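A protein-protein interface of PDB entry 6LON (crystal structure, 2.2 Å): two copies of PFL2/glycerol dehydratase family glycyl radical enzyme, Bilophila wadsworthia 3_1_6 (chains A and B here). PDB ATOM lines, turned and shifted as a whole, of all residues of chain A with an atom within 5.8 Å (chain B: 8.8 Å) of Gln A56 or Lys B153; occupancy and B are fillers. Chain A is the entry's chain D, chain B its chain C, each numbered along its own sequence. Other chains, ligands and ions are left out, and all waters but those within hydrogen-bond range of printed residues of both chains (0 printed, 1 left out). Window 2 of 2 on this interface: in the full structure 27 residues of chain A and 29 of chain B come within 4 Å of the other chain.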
ATOM      1  N   THR A  51      24.950 -17.426  -4.443  1.00  0.00           N
ATOM      2  CA  THR A  51      26.154 -16.797  -4.972  1.00  0.00           C
ATOM      3  C   THR A  51      25.812 -15.570  -5.798  1.00  0.00           C
ATOM      4  O   THR A  51      26.452 -14.512  -5.669  1.00  0.00           O
ATOM      5  CB  THR A  51      26.922 -17.819  -5.803  1.00  0.00           C
ATOM      6  OG1 THR A  51      27.384 -18.855  -4.935  1.00  0.00           O
ATOM      7  CG2 THR A  51      28.085 -17.191  -6.457  1.00  0.00           C
ATOM      8  N   GLU A  52      24.782 -15.693  -6.631  1.00  0.00           N
ATOM      9  CA  GLU A  52      24.360 -14.596  -7.494  1.00  0.00           C
ATOM     10  C   GLU A  52      24.100 -13.330  -6.700  1.00  0.00           C
ATOM     11  O   GLU A  52      24.484 -12.234  -7.120  1.00  0.00           O
ATOM     12  CB  GLU A  52      23.095 -15.010  -8.243  1.00  0.00           C
ATOM     13  CG  GLU A  52      22.609 -14.010  -9.243  1.00  0.00           C
ATOM     14  CD  GLU A  52      21.308 -14.477  -9.945  1.00  0.00           C
ATOM     15  OE1 GLU A  52      20.278 -14.672  -9.262  1.00  0.00           O
ATOM     16  OE2 GLU A  52      21.327 -14.675 -11.168  1.00  0.00           O
ATOM     17  N   SER A  53      23.437 -13.469  -5.547  1.00  0.00           N
ATOM     18  CA  SER A  53      23.152 -12.322  -4.687  1.00  0.00           C
ATOM     19  C   SER A  53      24.396 -11.862  -3.923  1.00  0.00           C
ATOM     20  O   SER A  53      24.716 -10.670  -3.923  1.00  0.00           O
ATOM     21  CB  SER A  53      22.000 -12.673  -3.724  1.00  0.00           C
ATOM     22  OG  SER A  53      21.808 -11.677  -2.739  1.00  0.00           O
ATOM     23  N   MET A  54      25.122 -12.791  -3.288  1.00  0.00           N
ATOM     24  CA  MET A  54      26.283 -12.407  -2.484  1.00  0.00           C
ATOM     25  C   MET A  54      27.286 -11.617  -3.307  1.00  0.00           C
ATOM     26  O   MET A  54      27.894 -10.656  -2.822  1.00  0.00           O
ATOM     27  CB  MET A  54      26.939 -13.658  -1.887  1.00  0.00           C
ATOM     28  CG  MET A  54      26.083 -14.328  -0.832  1.00  0.00           C
ATOM     29  SD  MET A  54      26.016 -13.357   0.714  1.00  0.00           S
ATOM     30  CE  MET A  54      27.610 -13.793   1.395  1.00  0.00           C
ATOM     31  N   ARG A  55      27.430 -11.984  -4.572  1.00  0.00           N
ATOM     32  CA  ARG A  55      28.323 -11.299  -5.498  1.00  0.00           C
ATOM     33  C   ARG A  55      28.000  -9.822  -5.640  1.00  0.00           C
ATOM     34  O   ARG A  55      28.891  -9.008  -5.916  1.00  0.00           O
ATOM     35  CB  ARG A  55      28.213 -12.032  -6.837  1.00  0.00           C
ATOM     36  CG  ARG A  55      29.094 -11.555  -7.897  1.00  0.00           C
ATOM     37  CD  ARG A  55      28.478 -11.904  -9.228  1.00  0.00           C
ATOM     38  NE  ARG A  55      28.459 -13.327  -9.487  1.00  0.00           N
ATOM     39  CZ  ARG A  55      29.508 -14.017  -9.934  1.00  0.00           C
ATOM     40  NH1 ARG A  55      30.682 -13.404 -10.134  1.00  0.00           N
ATOM     41  NH2 ARG A  55      29.381 -15.320 -10.189  1.00  0.00           N
ATOM     42  N   GLN A  56      26.768  -9.430  -5.407  1.00  0.00           N
ATOM     43  CA  GLN A  56      26.401  -8.042  -5.613  1.00  0.00           C
ATOM     44  C   GLN A  56      26.324  -7.214  -4.330  1.00  0.00           C
ATOM     45  O   GLN A  56      26.055  -6.014  -4.416  1.00  0.00           O
ATOM     46  CB  GLN A  56      25.065  -7.999  -6.356  1.00  0.00           C
ATOM     47  CG  GLN A  56      25.173  -8.587  -7.751  1.00  0.00           C
ATOM     48  CD  GLN A  56      23.874  -8.526  -8.490  1.00  0.00           C
ATOM     49  OE1 GLN A  56      23.000  -9.377  -8.308  1.00  0.00           O
ATOM     50  NE2 GLN A  56      23.733  -7.519  -9.338  1.00  0.00           N
ATOM     51  N   THR A  57      26.547  -7.811  -3.152  1.00  0.00           N
ATOM     52  CA  THR A  57      26.313  -7.131  -1.875  1.00  0.00           C
ATOM     53  C   THR A  57      27.568  -7.025  -1.015  1.00  0.00           C
ATOM     54  O   THR A  57      27.479  -6.621   0.152  1.00  0.00           O
ATOM     55  CB  THR A  57      25.200  -7.853  -1.128  1.00  0.00           C
ATOM     56  OG1 THR A  57      25.592  -9.195  -0.809  1.00  0.00           O
ATOM     57  CG2 THR A  57      23.985  -7.913  -2.006  1.00  0.00           C
ATOM     58  N   GLU A  58      28.736  -7.348  -1.579  1.00  0.00           N
ATOM     59  CA  GLU A  58      30.008  -7.288  -0.868  1.00  0.00           C
ATOM     60  C   GLU A  58      30.182  -5.964  -0.153  1.00  0.00           C
ATOM     61  O   GLU A  58      29.928  -4.905  -0.715  1.00  0.00           O
ATOM     62  CB  GLU A  58      31.159  -7.479  -1.852  1.00  0.00           C
ATOM     63  CG  GLU A  58      31.186  -8.861  -2.494  1.00  0.00           C
ATOM     64  CD  GLU A  58      32.427  -9.113  -3.357  1.00  0.00           C
ATOM     65  OE1 GLU A  58      33.288  -8.223  -3.495  1.00  0.00           O
ATOM     66  OE2 GLU A  58      32.543 -10.230  -3.884  1.00  0.00           O
ATOM     67  N   GLY A  59      30.618  -6.034   1.100  1.00  0.00           N
ATOM     68  CA  GLY A  59      30.896  -4.871   1.902  1.00  0.00           C
ATOM     69  C   GLY A  59      29.840  -4.584   2.942  1.00  0.00           C
ATOM     70  O   GLY A  59      30.149  -3.946   3.958  1.00  0.00           O
ATOM     71  N   GLU A  60      28.603  -5.053   2.713  1.00  0.00           N
ATOM     72  CA  GLU A  60      27.465  -4.816   3.584  1.00  0.00           C
ATOM     73  C   GLU A  60      27.515  -5.775   4.768  1.00  0.00           C
ATOM     74  O   GLU A  60      28.190  -6.803   4.730  1.00  0.00           O
ATOM     75  CB  GLU A  60      26.138  -5.013   2.835  1.00  0.00           C
ATOM     76  CG  GLU A  60      25.924  -4.039   1.701  1.00  0.00           C
ATOM     77  CD  GLU A  60      24.623  -4.289   0.905  1.00  0.00           C
ATOM     78  OE1 GLU A  60      23.819  -5.168   1.266  1.00  0.00           O
ATOM     79  OE2 GLU A  60      24.437  -3.600  -0.117  1.00  0.00           O
ATOM     80  N   TYR A 141      33.602 -17.403  -8.454  1.00  0.00           N
ATOM     81  CA  TYR A 141      33.286 -16.280  -7.580  1.00  0.00           C
ATOM     82  C   TYR A 141      33.933 -16.463  -6.205  1.00  0.00           C
ATOM     83  O   TYR A 141      34.478 -15.511  -5.642  1.00  0.00           O
ATOM     84  CB  TYR A 141      31.775 -16.085  -7.431  1.00  0.00           C
ATOM     85  CG  TYR A 141      31.544 -15.107  -6.324  1.00  0.00           C
ATOM     86  CD1 TYR A 141      31.771 -13.759  -6.529  1.00  0.00           C
ATOM     87  CD2 TYR A 141      31.215 -15.533  -5.042  1.00  0.00           C
ATOM     88  CE1 TYR A 141      31.639 -12.852  -5.522  1.00  0.00           C
ATOM     89  CE2 TYR A 141      31.064 -14.615  -4.000  1.00  0.00           C
ATOM     90  CZ  TYR A 141      31.277 -13.285  -4.243  1.00  0.00           C
ATOM     91  OH  TYR A 141      31.126 -12.379  -3.215  1.00  0.00           O
ATOM     92  N   ASP B 107      39.865   2.812  -7.825  1.00  0.00           N
ATOM     93  CA  ASP B 107      38.717   2.798  -8.718  1.00  0.00           C
ATOM     94  C   ASP B 107      38.560   4.094  -9.496  1.00  0.00           C
ATOM     95  O   ASP B 107      37.675   4.177 -10.354  1.00  0.00           O
ATOM     96  CB  ASP B 107      37.421   2.501  -7.935  1.00  0.00           C
ATOM     97  CG  ASP B 107      37.146   3.499  -6.784  1.00  0.00           C
ATOM     98  OD1 ASP B 107      38.082   4.037  -6.168  1.00  0.00           O
ATOM     99  OD2 ASP B 107      35.954   3.729  -6.480  1.00  0.00           O
ATOM    100  N   GLY B 144      37.112  -3.729  -6.753  1.00  0.00           N
ATOM    101  CA  GLY B 144      36.303  -4.282  -5.697  1.00  0.00           C
ATOM    102  C   GLY B 144      36.993  -4.340  -4.361  1.00  0.00           C
ATOM    103  O   GLY B 144      36.482  -4.982  -3.443  1.00  0.00           O
ATOM    104  N   THR B 146      38.915  -1.347  -2.965  1.00  0.00           N
ATOM    105  CA  THR B 146      39.426  -0.069  -2.500  1.00  0.00           C
ATOM    106  C   THR B 146      38.567   0.429  -1.347  1.00  0.00           C
ATOM    107  O   THR B 146      37.424   0.008  -1.173  1.00  0.00           O
ATOM    108  CB  THR B 146      39.451   0.982  -3.632  1.00  0.00           C
ATOM    109  OG1 THR B 146      38.115   1.289  -4.069  1.00  0.00           O
ATOM    110  CG2 THR B 146      40.320   0.514  -4.812  1.00  0.00           C
ATOM    111  N   TYR B 147      39.130   1.336  -0.548  1.00  0.00           N
ATOM    112  CA  TYR B 147      38.321   1.972   0.486  1.00  0.00           C
ATOM    113  C   TYR B 147      37.143   2.693  -0.143  1.00  0.00           C
ATOM    114  O   TYR B 147      36.004   2.556   0.313  1.00  0.00           O
ATOM    115  CB  TYR B 147      39.150   2.944   1.321  1.00  0.00           C
ATOM    116  CG  TYR B 147      38.314   3.752   2.266  1.00  0.00           C
ATOM    117  CD1 TYR B 147      37.811   3.187   3.421  1.00  0.00           C
ATOM    118  CD2 TYR B 147      38.018   5.074   1.990  1.00  0.00           C
ATOM    119  CE1 TYR B 147      37.046   3.917   4.285  1.00  0.00           C
ATOM    120  CE2 TYR B 147      37.254   5.829   2.839  1.00  0.00           C
ATOM    121  CZ  TYR B 147      36.775   5.253   4.003  1.00  0.00           C
ATOM    122  OH  TYR B 147      35.996   6.008   4.872  1.00  0.00           O
ATOM    123  N   HIS B 148      37.403   3.481  -1.189  1.00  0.00           N
ATOM    124  CA  HIS B 148      36.337   4.284  -1.779  1.00  0.00           C
ATOM    125  C   HIS B 148      35.163   3.425  -2.243  1.00  0.00           C
ATOM    126  O   HIS B 148      33.997   3.768  -1.999  1.00  0.00           O
ATOM    127  CB  HIS B 148      36.839   5.112  -2.962  1.00  0.00           C
ATOM    128  CG  HIS B 148      35.729   5.878  -3.606  1.00  0.00           C
ATOM    129  ND1 HIS B 148      35.193   5.535  -4.826  1.00  0.00           N
ATOM    130  CD2 HIS B 148      34.961   6.887  -3.131  1.00  0.00           C
ATOM    131  CE1 HIS B 148      34.184   6.344  -5.105  1.00  0.00           C
ATOM    132  NE2 HIS B 148      34.023   7.172  -4.090  1.00  0.00           N
ATOM    133  N   GLU B 149      35.451   2.314  -2.924  1.00  0.00           N
ATOM    134  CA  GLU B 149      34.384   1.416  -3.361  1.00  0.00           C
ATOM    135  C   GLU B 149      33.559   0.925  -2.186  1.00  0.00           C
ATOM    136  O   GLU B 149      32.323   0.838  -2.266  1.00  0.00           O
ATOM    137  CB  GLU B 149      34.979   0.222  -4.105  1.00  0.00           C
ATOM    138  CG  GLU B 149      35.287   0.478  -5.564  1.00  0.00           C
ATOM    139  CD  GLU B 149      36.247  -0.569  -6.129  1.00  0.00           C
ATOM    140  OE1 GLU B 149      37.407  -0.628  -5.645  1.00  0.00           O
ATOM    141  OE2 GLU B 149      35.843  -1.347  -7.024  1.00  0.00           O
ATOM    142  N   HIS B 150      34.230   0.574  -1.087  1.00  0.00           N
ATOM    143  CA  HIS B 150      33.520   0.064   0.079  1.00  0.00           C
ATOM    144  C   HIS B 150      32.598   1.133   0.661  1.00  0.00           C
ATOM    145  O   HIS B 150      31.402   0.895   0.872  1.00  0.00           O
ATOM    146  CB  HIS B 150      34.535  -0.426   1.111  1.00  0.00           C
ATOM    147  CG  HIS B 150      33.942  -1.297   2.167  1.00  0.00           C
ATOM    148  ND1 HIS B 150      34.702  -1.939   3.120  1.00  0.00           N
ATOM    149  CD2 HIS B 150      32.660  -1.618   2.433  1.00  0.00           C
ATOM    150  CE1 HIS B 150      33.915  -2.637   3.910  1.00  0.00           C
ATOM    151  NE2 HIS B 150      32.671  -2.467   3.509  1.00  0.00           N
ATOM    152  N   LEU B 151      33.139   2.323   0.928  1.00  0.00           N
ATOM    153  CA  LEU B 151      32.321   3.407   1.454  1.00  0.00           C
ATOM    154  C   LEU B 151      31.108   3.654   0.574  1.00  0.00           C
ATOM    155  O   LEU B 151      29.962   3.679   1.053  1.00  0.00           O
ATOM    156  CB  LEU B 151      33.165   4.673   1.568  1.00  0.00           C
ATOM    157  CG  LEU B 151      32.523   5.911   2.192  1.00  0.00           C
ATOM    158  CD1 LEU B 151      31.924   5.587   3.552  1.00  0.00           C
ATOM    159  CD2 LEU B 151      33.579   7.010   2.309  1.00  0.00           C
ATOM    160  N   ASN B 152      31.345   3.822  -0.725  1.00  0.00           N
ATOM    161  CA  ASN B 152      30.247   4.130  -1.626  1.00  0.00           C
ATOM    162  C   ASN B 152      29.214   3.031  -1.595  1.00  0.00           C
ATOM    163  O   ASN B 152      28.011   3.305  -1.526  1.00  0.00           O
ATOM    164  CB  ASN B 152      30.759   4.339  -3.044  1.00  0.00           C
ATOM    165  CG  ASN B 152      29.638   4.657  -4.015  1.00  0.00           C
ATOM    166  OD1 ASN B 152      29.003   5.710  -3.932  1.00  0.00           O
ATOM    167  ND2 ASN B 152      29.367   3.733  -4.919  1.00  0.00           N
ATOM    168  N   LYS B 153      29.665   1.781  -1.558  1.00  0.00           N
ATOM    169  CA  LYS B 153      28.727   0.667  -1.607  1.00  0.00           C
ATOM    170  C   LYS B 153      27.776   0.670  -0.417  1.00  0.00           C
ATOM    171  O   LYS B 153      26.571   0.463  -0.583  1.00  0.00           O
ATOM    172  CB  LYS B 153      29.482  -0.666  -1.670  1.00  0.00           C
ATOM    173  CG  LYS B 153      28.558  -1.859  -1.694  1.00  0.00           C
ATOM    174  CD  LYS B 153      27.396  -1.647  -2.685  1.00  0.00           C
ATOM    175  CE  LYS B 153      26.684  -2.951  -3.055  1.00  0.00           C
ATOM    176  NZ  LYS B 153      27.699  -3.912  -3.535  1.00  0.00           N
ATOM    177  N   VAL B 154      28.286   0.906   0.792  1.00  0.00           N
ATOM    178  CA  VAL B 154      27.500   0.639   1.996  1.00  0.00           C
ATOM    179  C   VAL B 154      26.800   1.855   2.541  1.00  0.00           C
ATOM    180  O   VAL B 154      26.012   1.719   3.481  1.00  0.00           O
ATOM    181  CB  VAL B 154      28.363   0.051   3.132  1.00  0.00           C
ATOM    182  CG1 VAL B 154      28.969  -1.282   2.690  1.00  0.00           C
ATOM    183  CG2 VAL B 154      29.426   1.069   3.564  1.00  0.00           C
ATOM    184  N   LEU B 155      27.072   3.033   2.022  1.00  0.00           N
ATOM    185  CA  LEU B 155      26.482   4.227   2.599  1.00  0.00           C
ATOM    186  C   LEU B 155      24.954   4.136   2.601  1.00  0.00           C
ATOM    187  O   LEU B 155      24.352   3.852   1.558  1.00  0.00           O
ATOM    188  CB  LEU B 155      26.959   5.431   1.806  1.00  0.00           C
ATOM    189  CG  LEU B 155      27.020   6.756   2.534  1.00  0.00           C
ATOM    190  CD1 LEU B 155      27.948   6.691   3.717  1.00  0.00           C
ATOM    191  CD2 LEU B 155      27.451   7.838   1.537  1.00  0.00           C
ATOM    192  N   PRO B 156      24.293   4.332   3.743  1.00  0.00           N
ATOM    193  CA  PRO B 156      22.824   4.284   3.756  1.00  0.00           C
ATOM    194  C   PRO B 156      22.241   5.267   2.767  1.00  0.00           C
ATOM    195  O   PRO B 156      22.788   6.350   2.534  1.00  0.00           O
ATOM    196  CB  PRO B 156      22.453   4.678   5.194  1.00  0.00           C
ATOM    197  CG  PRO B 156      23.684   4.423   6.006  1.00  0.00           C
ATOM    198  CD  PRO B 156      24.857   4.562   5.085  1.00  0.00           C
ATOM    199  N   ALA B 157      21.087   4.896   2.225  1.00  0.00           N
ATOM    200  CA  ALA B 157      20.422   5.741   1.239  1.00  0.00           C
ATOM    201  C   ALA B 157      20.116   7.116   1.815  1.00  0.00           C
ATOM    202  O   ALA B 157      20.271   8.139   1.136  1.00  0.00           O
ATOM    203  CB  ALA B 157      19.138   5.053   0.772  1.00  0.00           C
ATOM    204  N   ARG B 160      23.296   9.181   1.179  1.00  0.00           N
ATOM    205  CA  ARG B 160      23.945   9.329  -0.128  1.00  0.00           C
ATOM    206  C   ARG B 160      23.656  10.692  -0.750  1.00  0.00           C
ATOM    207  O   ARG B 160      24.548  11.323  -1.341  1.00  0.00           O
ATOM    208  CB  ARG B 160      23.464   8.249  -1.083  1.00  0.00           C
ATOM    209  CG  ARG B 160      23.905   6.884  -0.792  1.00  0.00           C
ATOM    210  CD  ARG B 160      23.600   6.038  -2.023  1.00  0.00           C
ATOM    211  NE  ARG B 160      24.380   6.531  -3.152  1.00  0.00           N
ATOM    212  CZ  ARG B 160      25.661   6.251  -3.328  1.00  0.00           C
ATOM    213  NH1 ARG B 160      26.292   5.480  -2.460  1.00  0.00           N
ATOM    214  NH2 ARG B 160      26.314   6.743  -4.360  1.00  0.00           N
ATOM    215  N   TYR B 164      27.263  12.105  -2.284  1.00  0.00           N
ATOM    216  CA  TYR B 164      27.689  11.731  -3.633  1.00  0.00           C
ATOM    217  C   TYR B 164      26.618  12.134  -4.637  1.00  0.00           C
ATOM    218  O   TYR B 164      25.420  11.962  -4.393  1.00  0.00           O
ATOM    219  CB  TYR B 164      27.955  10.210  -3.781  1.00  0.00           C
ATOM    220  CG  TYR B 164      29.145   9.701  -2.990  1.00  0.00           C
ATOM    221  CD1 TYR B 164      30.391  10.300  -3.094  1.00  0.00           C
ATOM    222  CD2 TYR B 164      29.015   8.632  -2.149  1.00  0.00           C
ATOM    223  CE1 TYR B 164      31.459   9.831  -2.397  1.00  0.00           C
ATOM    224  CE2 TYR B 164      30.082   8.162  -1.416  1.00  0.00           C
ATOM    225  CZ  TYR B 164      31.295   8.768  -1.538  1.00  0.00           C
ATOM    226  OH  TYR B 164      32.352   8.299  -0.806  1.00  0.00           O
ATOM    227  N   GLU B 167      25.988   7.405  -8.721  1.00  0.00           N
ATOM    228  CA  GLU B 167      25.791   6.101  -8.097  1.00  0.00           C
ATOM    229  C   GLU B 167      27.113   5.466  -7.717  1.00  0.00           C
ATOM    230  O   GLU B 167      27.167   4.700  -6.752  1.00  0.00           O
ATOM    231  CB  GLU B 167      25.000   5.170  -9.031  1.00  0.00           C
ATOM    232  N   ARG B 168      28.183   5.791  -8.434  1.00  0.00           N
ATOM    233  CA  ARG B 168      29.496   5.241  -8.171  1.00  0.00           C
ATOM    234  C   ARG B 168      30.331   6.105  -7.227  1.00  0.00           C
ATOM    235  O   ARG B 168      31.483   5.757  -6.941  1.00  0.00           O
ATOM    236  CB  ARG B 168      30.222   5.047  -9.495  1.00  0.00           C
ATOM    237  CG  ARG B 168      29.595   3.948 -10.344  1.00  0.00           C
ATOM    238  CD  ARG B 168      30.533   3.527 -11.474  1.00  0.00           C
ATOM    239  NE  ARG B 168      30.845   4.649 -12.353  1.00  0.00           N
ATOM    240  CZ  ARG B 168      31.981   4.791 -13.046  1.00  0.00           C
ATOM    241  NH1 ARG B 168      32.952   3.884 -12.962  1.00  0.00           N
ATOM    242  NH2 ARG B 168      32.157   5.867 -13.817  1.00  0.00           N
ATOM    243  N   GLY B 169      29.777   7.208  -6.732  1.00  0.00           N
ATOM    244  CA  GLY B 169      30.463   8.008  -5.734  1.00  0.00           C
ATOM    245  C   GLY B 169      31.754   8.639  -6.189  1.00  0.00           C
ATOM    246  O   GLY B 169      32.592   8.989  -5.346  1.00  0.00           O
ATOM    247  N   ILE B 540      30.473   5.929  10.136  1.00  0.00           N
ATOM    248  CA  ILE B 540      30.640   4.813   9.213  1.00  0.00           C
ATOM    249  C   ILE B 540      32.066   4.759   8.732  1.00  0.00           C
ATOM    250  O   ILE B 540      32.679   3.694   8.690  1.00  0.00           O
ATOM    251  CB  ILE B 540      29.651   4.939   8.043  1.00  0.00           C
ATOM    252  CG1 ILE B 540      28.239   4.742   8.559  1.00  0.00           C
ATOM    253  CG2 ILE B 540      29.998   3.966   6.936  1.00  0.00           C
ATOM    254  CD1 ILE B 540      27.176   5.407   7.715  1.00  0.00           C
ATOM    255  N   LEU B 544      34.742   1.691   8.804  1.00  0.00           N
ATOM    256  CA  LEU B 544      35.307   1.063   7.607  1.00  0.00           C
ATOM    257  C   LEU B 544      36.823   1.229   7.514  1.00  0.00           C
ATOM    258  O   LEU B 544      37.507   0.297   7.078  1.00  0.00           O
ATOM    259  CB  LEU B 544      34.653   1.647   6.353  1.00  0.00           C
ATOM    260  CG  LEU B 544      33.141   1.530   6.249  1.00  0.00           C
ATOM    261  CD1 LEU B 544      32.634   2.074   4.914  1.00  0.00           C
ATOM    262  CD2 LEU B 544      32.736   0.115   6.394  1.00  0.00           C
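No position is printed for both chains. Of the 7 pairs that touch across the chains among the printed residues, none has its exchanged pair printed and touching as well.
Of the printed residues of chain B, Gln A56 touches Lys B153 (2.8 Å). Of chain B, only Lys B153 comes within 4 Å of Thr A57. Printed residues of chain B within 4 Å of Glu A58: Lys B153. Of the printed residues of chain B, Gly A59 touches His B150 and Val B154. Of the printed residues of chain B, Glu A60 touches Lys B153 (3.8 Å) and Val B154 (3.8 Å). His B148 touches none of the printed residues of chain A. Of the printed residues of chain A, Lys B153 touches Gln A56, Thr A57, Glu A58 and Glu A60. Of the printed residues of chain A, Val B154 touches Gly A59 (3.2 Å) and Glu A60 (3.8 Å).
Of the 11 printed residues of chain A, 5 touch a printed residue of chain B. Printed residues of chain A that touch a printed residue of chain B: Gln A56, Thr A57, Glu A58, Gly A59 and Glu A60. Hydrophobic or aromatic side chains of chain B that line the printed part of chain A: His B150 and Val B154. Among the printed residues, 7 pairs touch across the chains. Among the printed residues, no Asp or Glu carboxylate lies within 4 Å of a Lys or Arg side-chain nitrogen of the other chain.
O of Gly A59 lies within hydrogen-bond range of NE2 of His B150. O of Gln A56 lies within hydrogen-bond range of NZ of Lys B153 (2.8 Å).
CA of Thr A57 touches NZ of Lys B153, at 3.9 Å. Lys B153 touches Glu A58. Gly A59 touches Val B154 (O to CG1, 3.2 Å). OE2 of Glu A60 touches CE of Lys B153, at 3.8 Å. CG1 of Val B154 touches N of Glu A60 (3.8 Å).
The backbone carbonyl oxygen (O) of Glu A52 lies close to the side-chain amide oxygen (OE1) of Gln A56 (3.4 Å). OH of Tyr A141 is in hydrogen-bond range of OE2 of Glu A58, 2.7 Å away. The backbone carbonyl oxygen of Met A54 lies within hydrogen-bond range of the side-chain hydroxyl of Thr A57 (3.4 Å).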
